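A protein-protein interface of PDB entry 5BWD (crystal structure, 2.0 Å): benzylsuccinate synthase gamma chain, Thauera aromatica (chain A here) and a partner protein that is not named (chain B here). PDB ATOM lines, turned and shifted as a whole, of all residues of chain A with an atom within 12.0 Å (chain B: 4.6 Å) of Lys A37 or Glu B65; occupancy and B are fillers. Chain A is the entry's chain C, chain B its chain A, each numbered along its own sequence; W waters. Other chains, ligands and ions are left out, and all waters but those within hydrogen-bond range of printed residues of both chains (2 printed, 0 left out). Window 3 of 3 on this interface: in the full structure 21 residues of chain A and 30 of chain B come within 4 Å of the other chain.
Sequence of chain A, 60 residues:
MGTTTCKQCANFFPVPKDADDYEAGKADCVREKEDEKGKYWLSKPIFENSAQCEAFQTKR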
ATOM      1  N   GLU A  32      10.864  12.202   1.170  1.00  0.00           N
ATOM      2  CA  GLU A  32      11.580  11.932  -0.072  1.00  0.00           C
ATOM      3  C   GLU A  32      10.600  11.892  -1.237  1.00  0.00           C
ATOM      4  O   GLU A  32       9.517  11.322  -1.126  1.00  0.00           O
ATOM      5  CB  GLU A  32      12.352  10.614   0.019  1.00  0.00           C
ATOM      6  CG  GLU A  32      13.022  10.198  -1.281  1.00  0.00           C
ATOM      7  CD  GLU A  32      13.832   8.928  -1.137  1.00  0.00           C
ATOM      8  OE1 GLU A  32      13.593   7.976  -1.913  1.00  0.00           O
ATOM      9  OE2 GLU A  32      14.711   8.883  -0.250  1.00  0.00           O
ATOM     10  N   LYS A  33      10.975  12.511  -2.350  1.00  0.00           N
ATOM     11  CA  LYS A  33      10.129  12.511  -3.536  1.00  0.00           C
ATOM     12  C   LYS A  33      10.959  12.217  -4.774  1.00  0.00           C
ATOM     13  O   LYS A  33      12.169  12.443  -4.786  1.00  0.00           O
ATOM     14  CB  LYS A  33       9.401  13.852  -3.691  1.00  0.00           C
ATOM     15  CG  LYS A  33       8.449  14.185  -2.546  1.00  0.00           C
ATOM     16  CD  LYS A  33       7.638  15.439  -2.837  1.00  0.00           C
ATOM     17  CE  LYS A  33       6.357  15.123  -3.595  1.00  0.00           C
ATOM     18  NZ  LYS A  33       5.339  14.472  -2.720  1.00  0.00           N
ATOM     19  N   GLU A  34      10.309  11.703  -5.811  1.00  0.00           N
ATOM     20  CA  GLU A  34      10.983  11.460  -7.079  1.00  0.00           C
ATOM     21  C   GLU A  34      10.014  11.609  -8.244  1.00  0.00           C
ATOM     22  O   GLU A  34       8.954  10.981  -8.266  1.00  0.00           O
ATOM     23  CB  GLU A  34      11.621  10.067  -7.095  1.00  0.00           C
ATOM     24  CG  GLU A  34      12.404   9.771  -8.365  1.00  0.00           C
ATOM     25  CD  GLU A  34      13.236   8.507  -8.266  1.00  0.00           C
ATOM     26  OE1 GLU A  34      12.902   7.629  -7.443  1.00  0.00           O
ATOM     27  OE2 GLU A  34      14.232   8.396  -9.014  1.00  0.00           O
ATOM     28  N   ASP A  35      10.373  12.456  -9.203  1.00  0.00           N
ATOM     29  CA  ASP A  35       9.590  12.594 -10.423  1.00  0.00           C
ATOM     30  C   ASP A  35      10.413  12.134 -11.620  1.00  0.00           C
ATOM     31  O   ASP A  35      11.325  11.320 -11.472  1.00  0.00           O
ATOM     32  CB  ASP A  35       9.108  14.038 -10.610  1.00  0.00           C
ATOM     33  CG  ASP A  35      10.223  15.062 -10.468  1.00  0.00           C
ATOM     34  OD1 ASP A  35      11.410  14.700 -10.627  1.00  0.00           O
ATOM     35  OD2 ASP A  35       9.902  16.240 -10.204  1.00  0.00           O
ATOM     36  N   GLU A  36      10.100  12.657 -12.800  1.00  0.00           N
ATOM     37  CA  GLU A  36      10.772  12.219 -14.020  1.00  0.00           C
ATOM     38  C   GLU A  36      12.215  12.716 -14.087  1.00  0.00           C
ATOM     39  O   GLU A  36      13.049  12.116 -14.767  1.00  0.00           O
ATOM     40  CB  GLU A  36      10.000  12.682 -15.262  1.00  0.00           C
ATOM     41  CG  GLU A  36       9.975  14.191 -15.480  1.00  0.00           C
ATOM     42  CD  GLU A  36       8.962  14.900 -14.600  1.00  0.00           C
ATOM     43  OE1 GLU A  36       8.243  14.215 -13.841  1.00  0.00           O
ATOM     44  OE2 GLU A  36       8.882  16.144 -14.670  1.00  0.00           O
ATOM     45  N   LYS A  37      12.507  13.807 -13.382  1.00  0.00           N
ATOM     46  CA  LYS A  37      13.855  14.372 -13.374  1.00  0.00           C
ATOM     47  C   LYS A  37      14.784  13.578 -12.465  1.00  0.00           C
ATOM     48  O   LYS A  37      15.861  13.157 -12.878  1.00  0.00           O
ATOM     49  CB  LYS A  37      13.830  15.836 -12.929  1.00  0.00           C
ATOM     50  CG  LYS A  37      13.163  16.778 -13.912  1.00  0.00           C
ATOM     51  CD  LYS A  37      13.771  16.637 -15.292  1.00  0.00           C
ATOM     52  CE  LYS A  37      13.137  17.605 -16.268  1.00  0.00           C
ATOM     53  NZ  LYS A  37      13.588  17.350 -17.665  1.00  0.00           N
ATOM     54  N   GLY A  38      14.364  13.385 -11.220  1.00  0.00           N
ATOM     55  CA  GLY A  38      15.173  12.664 -10.258  1.00  0.00           C
ATOM     56  C   GLY A  38      14.666  12.762  -8.832  1.00  0.00           C
ATOM     57  O   GLY A  38      13.537  13.187  -8.582  1.00  0.00           O
ATOM     58  N   LYS A  39      15.518  12.373  -7.892  1.00  0.00           N
ATOM     59  CA  LYS A  39      15.139  12.293  -6.490  1.00  0.00           C
ATOM     60  C   LYS A  39      15.489  13.571  -5.735  1.00  0.00           C
ATOM     61  O   LYS A  39      16.475  14.242  -6.047  1.00  0.00           O
ATOM     62  CB  LYS A  39      15.821  11.089  -5.836  1.00  0.00           C
ATOM     63  CG  LYS A  39      15.391  10.815  -4.410  1.00  0.00           C
ATOM     64  CD  LYS A  39      16.038   9.547  -3.880  1.00  0.00           C
ATOM     65  CE  LYS A  39      15.629   8.332  -4.694  1.00  0.00           C
ATOM     66  NZ  LYS A  39      16.187   7.077  -4.116  1.00  0.00           N
ATOM     67  N   TYR A  40      14.669  13.911  -4.747  1.00  0.00           N
ATOM     68  CA  TYR A  40      14.970  15.039  -3.874  1.00  0.00           C
ATOM     69  C   TYR A  40      14.257  14.907  -2.537  1.00  0.00           C
ATOM     70  O   TYR A  40      13.373  14.067  -2.373  1.00  0.00           O
ATOM     71  CB  TYR A  40      14.602  16.364  -4.549  1.00  0.00           C
ATOM     72  CG  TYR A  40      13.133  16.557  -4.848  1.00  0.00           C
ATOM     73  CD1 TYR A  40      12.574  16.076  -6.025  1.00  0.00           C
ATOM     74  CD2 TYR A  40      12.309  17.249  -3.966  1.00  0.00           C
ATOM     75  CE1 TYR A  40      11.233  16.261  -6.308  1.00  0.00           C
ATOM     76  CE2 TYR A  40      10.968  17.439  -4.239  1.00  0.00           C
ATOM     77  CZ  TYR A  40      10.437  16.947  -5.413  1.00  0.00           C
ATOM     78  OH  TYR A  40       9.105  17.140  -5.691  1.00  0.00           O
ATOM     79  N   TRP A  41      14.652  15.740  -1.581  1.00  0.00           N
ATOM     80  CA  TRP A  41      14.083  15.689  -0.240  1.00  0.00           C
ATOM     81  C   TRP A  41      13.574  17.058   0.207  1.00  0.00           C
ATOM     82  O   TRP A  41      14.188  18.089  -0.083  1.00  0.00           O
ATOM     83  CB  TRP A  41      15.120  15.156   0.749  1.00  0.00           C
ATOM     84  CG  TRP A  41      15.579  13.764   0.419  1.00  0.00           C
ATOM     85  CD1 TRP A  41      15.068  12.599   0.907  1.00  0.00           C
ATOM     86  CD2 TRP A  41      16.630  13.393  -0.484  1.00  0.00           C
ATOM     87  NE1 TRP A  41      15.737  11.522   0.370  1.00  0.00           N
ATOM     88  CE2 TRP A  41      16.703  11.984  -0.486  1.00  0.00           C
ATOM     89  CE3 TRP A  41      17.519  14.114  -1.287  1.00  0.00           C
ATOM     90  CZ2 TRP A  41      17.626  11.284  -1.259  1.00  0.00           C
ATOM     91  CZ3 TRP A  41      18.435  13.419  -2.053  1.00  0.00           C
ATOM     92  CH2 TRP A  41      18.483  12.015  -2.034  1.00  0.00           C
ATOM     93  N   ARG B  52      19.366  15.782 -16.208  1.00  0.00           N
ATOM     94  CA  ARG B  52      18.180  15.834 -15.353  1.00  0.00           C
ATOM     95  C   ARG B  52      17.898  17.247 -14.832  1.00  0.00           C
ATOM     96  O   ARG B  52      17.123  17.429 -13.887  1.00  0.00           O
ATOM     97  CB  ARG B  52      18.324  14.864 -14.176  1.00  0.00           C
ATOM     98  CG  ARG B  52      19.207  15.359 -13.033  1.00  0.00           C
ATOM     99  CD  ARG B  52      18.484  15.195 -11.703  1.00  0.00           C
ATOM    100  NE  ARG B  52      19.226  15.755 -10.574  1.00  0.00           N
ATOM    101  CZ  ARG B  52      19.148  17.025 -10.186  1.00  0.00           C
ATOM    102  NH1 ARG B  52      19.847  17.448  -9.143  1.00  0.00           N
ATOM    103  NH2 ARG B  52      18.369  17.875 -10.844  1.00  0.00           N
ATOM    104  N   CYS B  53      18.511  18.245 -15.459  1.00  0.00           N
ATOM    105  CA  CYS B  53      18.352  19.635 -15.031  1.00  0.00           C
ATOM    106  C   CYS B  53      16.884  20.056 -15.036  1.00  0.00           C
ATOM    107  O   CYS B  53      16.151  19.787 -15.988  1.00  0.00           O
ATOM    108  CB  CYS B  53      19.169  20.567 -15.927  1.00  0.00           C
ATOM    109  SG  CYS B  53      19.225  22.297 -15.382  1.00  0.00           S
ATOM    110  N   ARG B  54      16.459  20.706 -13.958  1.00  0.00           N
ATOM    111  CA  ARG B  54      15.086  21.180 -13.850  1.00  0.00           C
ATOM    112  C   ARG B  54      14.954  22.537 -14.522  1.00  0.00           C
ATOM    113  O   ARG B  54      14.856  23.563 -13.853  1.00  0.00           O
ATOM    114  CB  ARG B  54      14.658  21.258 -12.386  1.00  0.00           C
ATOM    115  CG  ARG B  54      14.675  19.909 -11.685  1.00  0.00           C
ATOM    116  CD  ARG B  54      14.131  19.992 -10.268  1.00  0.00           C
ATOM    117  NE  ARG B  54      14.204  18.693  -9.610  1.00  0.00           N
ATOM    118  CZ  ARG B  54      13.290  17.739  -9.745  1.00  0.00           C
ATOM    119  NH1 ARG B  54      12.228  17.942 -10.510  1.00  0.00           N
ATOM    120  NH2 ARG B  54      13.441  16.579  -9.118  1.00  0.00           N
ATOM    121  N   TRP B  55      14.963  22.529 -15.851  1.00  0.00           N
ATOM    122  CA  TRP B  55      14.944  23.757 -16.634  1.00  0.00           C
ATOM    123  C   TRP B  55      13.721  24.615 -16.318  1.00  0.00           C
ATOM    124  O   TRP B  55      12.613  24.106 -16.141  1.00  0.00           O
ATOM    125  CB  TRP B  55      14.982  23.438 -18.128  1.00  0.00           C
ATOM    126  CG  TRP B  55      16.102  22.528 -18.543  1.00  0.00           C
ATOM    127  CD1 TRP B  55      16.005  21.204 -18.860  1.00  0.00           C
ATOM    128  CD2 TRP B  55      17.488  22.875 -18.690  1.00  0.00           C
ATOM    129  NE1 TRP B  55      17.241  20.706 -19.197  1.00  0.00           N
ATOM    130  CE2 TRP B  55      18.169  21.711 -19.099  1.00  0.00           C
ATOM    131  CE3 TRP B  55      18.218  24.056 -18.515  1.00  0.00           C
ATOM    132  CZ2 TRP B  55      19.545  21.691 -19.336  1.00  0.00           C
ATOM    133  CZ3 TRP B  55      19.582  24.037 -18.749  1.00  0.00           C
ATOM    134  CH2 TRP B  55      20.232  22.860 -19.156  1.00  0.00           C
ATOM    135  N   PHE B  63       5.961  27.315 -19.902  1.00  0.00           N
ATOM    136  CA  PHE B  63       7.227  26.695 -19.533  1.00  0.00           C
ATOM    137  C   PHE B  63       7.455  25.422 -20.332  1.00  0.00           C
ATOM    138  O   PHE B  63       6.512  24.711 -20.669  1.00  0.00           O
ATOM    139  CB  PHE B  63       7.267  26.394 -18.035  1.00  0.00           C
ATOM    140  CG  PHE B  63       7.250  27.622 -17.169  1.00  0.00           C
ATOM    141  CD1 PHE B  63       8.391  28.396 -17.017  1.00  0.00           C
ATOM    142  CD2 PHE B  63       6.094  28.000 -16.504  1.00  0.00           C
ATOM    143  CE1 PHE B  63       8.377  29.529 -16.221  1.00  0.00           C
ATOM    144  CE2 PHE B  63       6.074  29.129 -15.706  1.00  0.00           C
ATOM    145  CZ  PHE B  63       7.216  29.896 -15.564  1.00  0.00           C
ATOM    146  N   ILE B  64       8.716  25.139 -20.635  1.00  0.00           N
ATOM    147  CA  ILE B  64       9.053  23.984 -21.450  1.00  0.00           C
ATOM    148  C   ILE B  64       8.991  22.716 -20.608  1.00  0.00           C
ATOM    149  O   ILE B  64       8.607  21.655 -21.097  1.00  0.00           O
ATOM    150  CB  ILE B  64      10.422  24.172 -22.111  1.00  0.00           C
ATOM    151  CG1 ILE B  64      10.420  25.484 -22.897  1.00  0.00           C
ATOM    152  CG2 ILE B  64      10.755  22.989 -23.006  1.00  0.00           C
ATOM    153  CD1 ILE B  64      11.407  25.539 -24.019  1.00  0.00           C
ATOM    154  N   GLU B  65       9.355  22.832 -19.336  1.00  0.00           N
ATOM    155  CA  GLU B  65       9.173  21.732 -18.400  1.00  0.00           C
ATOM    156  C   GLU B  65       7.765  21.796 -17.818  1.00  0.00           C
ATOM    157  O   GLU B  65       7.277  22.872 -17.467  1.00  0.00           O
ATOM    158  CB  GLU B  65      10.228  21.774 -17.293  1.00  0.00           C
ATOM    159  CG  GLU B  65      11.636  21.465 -17.778  1.00  0.00           C
ATOM    160  CD  GLU B  65      11.763  20.059 -18.346  1.00  0.00           C
ATOM    161  OE1 GLU B  65      10.987  19.174 -17.928  1.00  0.00           O
ATOM    162  OE2 GLU B  65      12.637  19.841 -19.210  1.00  0.00           O
ATOM    163  N   LYS B  66       7.115  20.643 -17.715  1.00  0.00           N
ATOM    164  CA  LYS B  66       5.684  20.601 -17.418  1.00  0.00           C
ATOM    165  C   LYS B  66       5.331  20.843 -15.948  1.00  0.00           C
ATOM    166  O   LYS B  66       4.211  21.247 -15.640  1.00  0.00           O
ATOM    167  CB  LYS B  66       5.099  19.258 -17.875  1.00  0.00           C
ATOM    168  CG  LYS B  66       5.783  18.025 -17.291  1.00  0.00           C
ATOM    169  CD  LYS B  66       5.368  16.770 -18.053  1.00  0.00           C
ATOM    170  CE  LYS B  66       5.922  15.502 -17.419  1.00  0.00           C
ATOM    171  NZ  LYS B  66       5.117  15.052 -16.250  1.00  0.00           N
ATOM    172  N   SER B  67       6.272  20.597 -15.044  1.00  0.00           N
ATOM    173  CA  SER B  67       5.981  20.702 -13.613  1.00  0.00           C
ATOM    174  C   SER B  67       6.170  22.118 -13.061  1.00  0.00           C
ATOM    175  O   SER B  67       5.854  22.383 -11.899  1.00  0.00           O
ATOM    176  CB  SER B  67       6.860  19.727 -12.826  1.00  0.00           C
ATOM    177  OG  SER B  67       6.550  18.385 -13.158  1.00  0.00           O
ATOM    178  N   VAL B  68       6.683  23.021 -13.892  1.00  0.00           N
ATOM    179  CA  VAL B  68       6.984  24.378 -13.447  1.00  0.00           C
ATOM    180  C   VAL B  68       5.699  25.152 -13.181  1.00  0.00           C
ATOM    181  O   VAL B  68       4.844  25.270 -14.058  1.00  0.00           O
ATOM    182  CB  VAL B  68       7.862  25.115 -14.466  1.00  0.00           C
ATOM    183  CG1 VAL B  68       8.215  26.506 -13.958  1.00  0.00           C
ATOM    184  CG2 VAL B  68       9.130  24.312 -14.745  1.00  0.00           C
HETATM  185  O   HOH W   1      16.202  17.800 -17.878  1.00  0.00           O
HETATM  186  O   HOH W   2      16.105  15.764  -8.334  1.00  0.00           O
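Along chain A the printed residues that touch a printed residue of chain B span positions 35 to 40. Of the 10 printed residues of chain B, 5 touch a printed residue of chain A. Printed residues of chain B that touch a printed residue of chain A: Arg B52, Cys B53, Arg B54, Glu B65 and Ser B67.
Water W1 lies within hydrogen-bond range of the side-chain amino group of Lys A37 (2.7 Å), the backbone carbonyl oxygen of Cys B53 (2.7 Å) and the indole nitrogen of Trp B55 (3.4 Å). Water W2 lies within hydrogen-bond range of O of Lys A39 (2.8 Å) and NH2 of Arg B54 (2.9 Å).
Among the printed residues, merely in contact across the chains: Tyr A40 with Arg B54 (3.3 Å), Lys A37 with Arg B52 (3.3 Å), Glu A36 with Ser B67 (3.6 Å), Lys A37 with Arg B54 (3.6 Å) and Lys A37 with Cys B53 (3.7 Å).
The side-chain carboxylate (OD1) of Asp A35 lies within hydrogen-bond range of the backbone NH (N) of Lys A37, 3.1 Å away. The backbone NH of Lys A33 lies within hydrogen-bond range of the backbone carbonyl oxygen of Tyr A40, at 2.9 Å. The side-chain carboxylate of Asp A35 sits at hydrogen-bond distance from the backbone NH of Gly A38 (3.3 Å).
Printed residues of chain B within 4 Å of Asp A35: Arg B54 (2.9 Å). Printed residues of chain B within 4 Å of Glu A36: Ser B67 (3.6 Å). Lys A37 touches just these residues of chain B: Arg B52 (3.3 Å), Cys B53 (3.7 Å), Arg B54 (3.6 Å) and Glu B65 (3.1 Å). Of the printed residues of chain B, Gly A38 touches Arg B54. Lys A39 touches none of the printed residues of chain B. Of the printed residues of chain B, Tyr A40 touches Arg B54 (3.3 Å). Trp A41 touches none of the printed residues of chain B. Printed residues of chain A within 4 Å of Arg B52: Lys A37. Arg B54 touches four residues of chain A. No residue of chain A comes within 4 Å of Phe B63. No residue of chain A comes within 4 Å of Ile B64. Glu B65 touches one residue of chain A. Lys B66 touches none of the printed residues of chain A. Of chain A, only Glu A36 (3.6 Å) comes within 4 Å of Ser B67. No residue of chain A comes within 4 Å of Val B68. The nearest printed residue of chain B that does not touch Lys A37 is Trp B55 (4.7 Å).
NH2 of Arg B54 is in hydrogen-bond range of O of Gly A38. The side-chain amino group of Lys A37 is in salt-bridge range of the side-chain carboxylate of Glu B65, 3.1 Å away. NH1 of Arg B54 lies within salt-bridge range of OD2 of Asp A35 (2.9 Å).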
